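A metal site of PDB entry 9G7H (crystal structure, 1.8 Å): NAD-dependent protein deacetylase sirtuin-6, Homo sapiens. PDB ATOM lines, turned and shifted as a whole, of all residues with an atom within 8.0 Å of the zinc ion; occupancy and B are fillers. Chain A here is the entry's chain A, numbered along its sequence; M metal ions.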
ATOM      1  N   GLU A 134       2.657  28.524  -9.719  1.00  0.00           N
ATOM      2  CA  GLU A 134       3.236  27.196  -9.630  1.00  0.00           C
ATOM      3  C   GLU A 134       3.258  26.758  -8.165  1.00  0.00           C
ATOM      4  O   GLU A 134       3.652  27.551  -7.323  1.00  0.00           O
ATOM      5  CB  GLU A 134       4.675  27.202 -10.165  1.00  0.00           C
ATOM      6  CG  GLU A 134       5.354  25.837 -10.089  1.00  0.00           C
ATOM      7  CD  GLU A 134       6.709  25.690 -10.787  1.00  0.00           C
ATOM      8  OE1 GLU A 134       6.820  26.040 -11.981  1.00  0.00           O
ATOM      9  OE2 GLU A 134       7.646  25.174 -10.137  1.00  0.00           O
ATOM     10  N   CYS A 135       2.916  25.499  -7.882  1.00  0.00           N
ATOM     11  CA  CYS A 135       2.964  24.946  -6.527  1.00  0.00           C
ATOM     12  C   CYS A 135       4.418  24.635  -6.122  1.00  0.00           C
ATOM     13  O   CYS A 135       5.119  23.907  -6.819  1.00  0.00           O
ATOM     14  CB  CYS A 135       2.139  23.664  -6.456  1.00  0.00           C
ATOM     15  SG  CYS A 135       2.063  22.901  -4.809  1.00  0.00           S
ATOM     16  N   ALA A 136       4.854  25.166  -4.975  1.00  0.00           N
ATOM     17  CA  ALA A 136       6.193  24.921  -4.461  1.00  0.00           C
ATOM     18  C   ALA A 136       6.360  23.466  -4.004  1.00  0.00           C
ATOM     19  O   ALA A 136       7.466  22.937  -4.047  1.00  0.00           O
ATOM     20  CB  ALA A 136       6.516  25.882  -3.351  1.00  0.00           C
ATOM     21  N   LYS A 137       5.251  22.809  -3.608  1.00  0.00           N
ATOM     22  CA  LYS A 137       5.301  21.401  -3.244  1.00  0.00           C
ATOM     23  C   LYS A 137       5.349  20.501  -4.475  1.00  0.00           C
ATOM     24  O   LYS A 137       6.399  19.914  -4.755  1.00  0.00           O
ATOM     25  CB  LYS A 137       4.111  20.984  -2.371  1.00  0.00           C
ATOM     26  CG  LYS A 137       3.986  21.722  -1.054  1.00  0.00           C
ATOM     27  CD  LYS A 137       3.103  21.002  -0.040  1.00  0.00           C
ATOM     28  CE  LYS A 137       3.652  21.111   1.354  1.00  0.00           C
ATOM     29  NZ  LYS A 137       2.669  20.711   2.371  1.00  0.00           N
ATOM     30  N   CYS A 138       4.241  20.389  -5.223  1.00  0.00           N
ATOM     31  CA  CYS A 138       4.101  19.399  -6.283  1.00  0.00           C
ATOM     32  C   CYS A 138       4.562  19.893  -7.650  1.00  0.00           C
ATOM     33  O   CYS A 138       4.719  19.091  -8.555  1.00  0.00           O
ATOM     34  CB  CYS A 138       2.667  18.876  -6.362  1.00  0.00           C
ATOM     35  SG  CYS A 138       1.486  20.095  -7.007  1.00  0.00           S
ATOM     36  N   LYS A 139       4.773  21.211  -7.813  1.00  0.00           N
ATOM     37  CA  LYS A 139       5.289  21.784  -9.053  1.00  0.00           C
ATOM     38  C   LYS A 139       4.233  21.844 -10.152  1.00  0.00           C
ATOM     39  O   LYS A 139       4.563  22.186 -11.289  1.00  0.00           O
ATOM     40  CB  LYS A 139       6.527  21.047  -9.570  1.00  0.00           C
ATOM     41  CG  LYS A 139       7.608  20.786  -8.530  1.00  0.00           C
ATOM     42  CD  LYS A 139       8.185  22.040  -7.888  1.00  0.00           C
ATOM     43  CE  LYS A 139       9.257  21.687  -6.917  1.00  0.00           C
ATOM     44  NZ  LYS A 139      10.196  22.785  -6.730  1.00  0.00           N
ATOM     45  N   THR A 140       2.960  21.537  -9.831  1.00  0.00           N
ATOM     46  CA  THR A 140       1.886  21.656 -10.805  1.00  0.00           C
ATOM     47  C   THR A 140       1.679  23.140 -11.103  1.00  0.00           C
ATOM     48  O   THR A 140       1.665  23.957 -10.185  1.00  0.00           O
ATOM     49  CB  THR A 140       0.605  21.006 -10.292  1.00  0.00           C
ATOM     50  OG1 THR A 140       0.978  19.674  -9.930  1.00  0.00           O
ATOM     51  CG2 THR A 140      -0.495  20.970 -11.341  1.00  0.00           C
ATOM     52  N   GLN A 141       1.554  23.472 -12.399  1.00  0.00           N
ATOM     53  CA  GLN A 141       1.348  24.852 -12.827  1.00  0.00           C
ATOM     54  C   GLN A 141      -0.117  25.118 -13.145  1.00  0.00           C
ATOM     55  O   GLN A 141      -0.853  24.260 -13.616  1.00  0.00           O
ATOM     56  CB  GLN A 141       2.171  25.260 -14.037  1.00  0.00           C
ATOM     57  CG  GLN A 141       3.628  25.537 -13.695  1.00  0.00           C
ATOM     58  CD  GLN A 141       4.581  25.644 -14.868  1.00  0.00           C
ATOM     59  OE1 GLN A 141       4.258  25.385 -16.016  1.00  0.00           O
ATOM     60  NE2 GLN A 141       5.793  26.104 -14.568  1.00  0.00           N
ATOM     61  N   TYR A 142      -0.506  26.372 -12.951  1.00  0.00           N
ATOM     62  CA  TYR A 142      -1.865  26.823 -13.185  1.00  0.00           C
ATOM     63  C   TYR A 142      -1.767  28.060 -14.059  1.00  0.00           C
ATOM     64  O   TYR A 142      -1.015  28.991 -13.732  1.00  0.00           O
ATOM     65  CB  TYR A 142      -2.594  27.258 -11.911  1.00  0.00           C
ATOM     66  CG  TYR A 142      -2.803  26.161 -10.883  1.00  0.00           C
ATOM     67  CD1 TYR A 142      -1.748  25.710 -10.102  1.00  0.00           C
ATOM     68  CD2 TYR A 142      -4.054  25.631 -10.655  1.00  0.00           C
ATOM     69  CE1 TYR A 142      -1.926  24.717  -9.163  1.00  0.00           C
ATOM     70  CE2 TYR A 142      -4.263  24.669  -9.691  1.00  0.00           C
ATOM     71  CZ  TYR A 142      -3.197  24.194  -8.942  1.00  0.00           C
ATOM     72  OH  TYR A 142      -3.481  23.245  -7.994  1.00  0.00           O
ATOM     73  N   LEU A 159      -3.808  28.473  -2.859  1.00  0.00           N
ATOM     74  CA  LEU A 159      -3.220  27.174  -2.560  1.00  0.00           C
ATOM     75  C   LEU A 159      -3.529  26.190  -3.679  1.00  0.00           C
ATOM     76  O   LEU A 159      -4.468  26.370  -4.451  1.00  0.00           O
ATOM     77  CB  LEU A 159      -3.689  26.615  -1.219  1.00  0.00           C
ATOM     78  CG  LEU A 159      -3.400  27.484   0.007  1.00  0.00           C
ATOM     79  CD1 LEU A 159      -4.149  26.832   1.185  1.00  0.00           C
ATOM     80  CD2 LEU A 159      -1.896  27.627   0.273  1.00  0.00           C
ATOM     81  N   CYS A 160      -2.734  25.120  -3.691  1.00  0.00           N
ATOM     82  CA  CYS A 160      -2.803  24.096  -4.714  1.00  0.00           C
ATOM     83  C   CYS A 160      -4.063  23.244  -4.526  1.00  0.00           C
ATOM     84  O   CYS A 160      -4.385  22.886  -3.403  1.00  0.00           O
ATOM     85  CB  CYS A 160      -1.567  23.228  -4.614  1.00  0.00           C
ATOM     86  SG  CYS A 160      -1.395  22.112  -6.027  1.00  0.00           S
ATOM     87  N   THR A 161      -4.764  22.927  -5.633  1.00  0.00           N
ATOM     88  CA  THR A 161      -6.025  22.196  -5.558  1.00  0.00           C
ATOM     89  C   THR A 161      -5.851  20.766  -6.079  1.00  0.00           C
ATOM     90  O   THR A 161      -6.848  20.086  -6.258  1.00  0.00           O
ATOM     91  CB  THR A 161      -7.116  22.915  -6.347  1.00  0.00           C
ATOM     92  OG1 THR A 161      -6.901  22.747  -7.740  1.00  0.00           O
ATOM     93  CG2 THR A 161      -7.212  24.395  -6.005  1.00  0.00           C
ATOM     94  N   VAL A 162      -4.616  20.302  -6.301  1.00  0.00           N
ATOM     95  CA  VAL A 162      -4.402  18.995  -6.918  1.00  0.00           C
ATOM     96  C   VAL A 162      -5.084  17.929  -6.050  1.00  0.00           C
ATOM     97  O   VAL A 162      -4.957  17.947  -4.828  1.00  0.00           O
ATOM     98  CB  VAL A 162      -2.917  18.648  -7.160  1.00  0.00           C
ATOM     99  CG1 VAL A 162      -2.722  17.175  -7.491  1.00  0.00           C
ATOM    100  CG2 VAL A 162      -2.292  19.510  -8.242  1.00  0.00           C
ATOM    101  N   ALA A 163      -5.785  16.990  -6.711  1.00  0.00           N
ATOM    102  CA  ALA A 163      -6.626  15.991  -6.062  1.00  0.00           C
ATOM    103  C   ALA A 163      -5.875  15.321  -4.910  1.00  0.00           C
ATOM    104  O   ALA A 163      -5.639  14.105  -5.033  1.00  0.00           O
ATOM    105  CB  ALA A 163      -7.081  14.973  -7.097  1.00  0.00           C
ATOM    106  N   CYS A 171      -3.308  18.704  -2.203  1.00  0.00           N
ATOM    107  CA  CYS A 171      -1.896  19.074  -1.932  1.00  0.00           C
ATOM    108  C   CYS A 171      -1.840  20.292  -1.002  1.00  0.00           C
ATOM    109  O   CYS A 171      -1.130  20.260  -0.009  1.00  0.00           O
ATOM    110  CB  CYS A 171      -1.150  19.286  -3.239  1.00  0.00           C
ATOM    111  SG  CYS A 171       0.366  20.262  -3.026  1.00  0.00           S
ATOM    112  N   ARG A 172      -2.570  21.356  -1.368  1.00  0.00           N
ATOM    113  CA  ARG A 172      -2.704  22.562  -0.547  1.00  0.00           C
ATOM    114  C   ARG A 172      -1.371  23.303  -0.417  1.00  0.00           C
ATOM    115  O   ARG A 172      -1.181  24.115   0.488  1.00  0.00           O
ATOM    116  CB  ARG A 172      -3.358  22.276   0.818  1.00  0.00           C
ATOM    117  CG  ARG A 172      -4.554  21.339   0.765  1.00  0.00           C
ATOM    118  CD  ARG A 172      -5.720  21.686   1.697  1.00  0.00           C
ATOM    119  NE  ARG A 172      -5.353  22.459   2.889  1.00  0.00           N
ATOM    120  CZ  ARG A 172      -5.732  23.718   3.150  1.00  0.00           C
ATOM    121  NH1 ARG A 172      -6.560  24.370   2.351  1.00  0.00           N
ATOM    122  NH2 ARG A 172      -5.258  24.343   4.204  1.00  0.00           N
ATOM    123  N   GLY A 173      -0.483  23.097  -1.387  1.00  0.00           N
ATOM    124  CA  GLY A 173       0.789  23.789  -1.420  1.00  0.00           C
ATOM    125  C   GLY A 173       0.614  25.266  -1.778  1.00  0.00           C
ATOM    126  O   GLY A 173      -0.359  25.622  -2.447  1.00  0.00           O
ATOM    127  N   GLU A 174       1.565  26.083  -1.325  1.00  0.00           N
ATOM    128  CA  GLU A 174       1.590  27.521  -1.525  1.00  0.00           C
ATOM    129  C   GLU A 174       1.868  27.825  -2.996  1.00  0.00           C
ATOM    130  O   GLU A 174       2.926  27.438  -3.490  1.00  0.00           O
ATOM    131  CB  GLU A 174       2.720  28.094  -0.666  1.00  0.00           C
ATOM    132  CG  GLU A 174       2.713  29.616  -0.532  1.00  0.00           C
ATOM    133  CD  GLU A 174       3.789  30.150   0.416  1.00  0.00           C
ATOM    134  OE1 GLU A 174       3.409  30.714   1.467  1.00  0.00           O
ATOM    135  OE2 GLU A 174       4.998  30.044   0.078  1.00  0.00           O
ATOM    136  N   LEU A 175       0.920  28.500  -3.677  1.00  0.00           N
ATOM    137  CA  LEU A 175       1.133  28.934  -5.051  1.00  0.00           C
ATOM    138  C   LEU A 175       2.065  30.165  -5.094  1.00  0.00           C
ATOM    139  O   LEU A 175       1.996  31.080  -4.274  1.00  0.00           O
ATOM    140  CB  LEU A 175      -0.242  29.176  -5.690  1.00  0.00           C
ATOM    141  CG  LEU A 175      -1.129  27.936  -5.826  1.00  0.00           C
ATOM    142  CD1 LEU A 175      -2.263  28.085  -6.855  1.00  0.00           C
ATOM    143  CD2 LEU A 175      -0.210  26.750  -6.145  1.00  0.00           C
HETATM  144 ZN    ZN M   1       0.583  21.160  -5.217  1.00  0.00          ZN
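OG1 of Thr 140 lies close to SG of Cys 138 (3.0 Å). The side-chain sulfur (SG) of Cys 135 sits close to the backbone NH (N) of Lys 137. The backbone NH (N) of Cys 135 lies within hydrogen-bond range of the backbone carbonyl oxygen (O) of Thr 140, 3.0 Å away. N of Cys 160 lies within hydrogen-bond range of O of Gly 173 (2.7 Å). The side-chain sulfur (SG) of Cys 160 sits close to the backbone NH (N) of Val 162, at 3.7 Å. The backbone carbonyl oxygen (O) of Cys 160 is in hydrogen-bond range of the backbone NH (N) of Arg 172 (3.1 Å). SG of Cys 160 lies close to OH of Tyr 142. The side-chain sulfur (SG) of Cys 171 sits close to the backbone NH (N) of Gly 173, 3.4 Å away.
Within 4 Å of the zinc ion: Cys 135, Cys 138, Cys 160 and Cys 171. The nearest printed residue that does not touch the zinc ion is Gly 173 (4.4 Å).
SG of Cys 138 is bound to the zinc ion. The zinc ion is bound by SG of Cys 135 (2.3 Å). The zinc ion is bound by SG of Cys 160, 2.3 Å away. SG of Cys 171 is bound to the zinc ion. The zinc ion has four donor atoms within binding distance.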
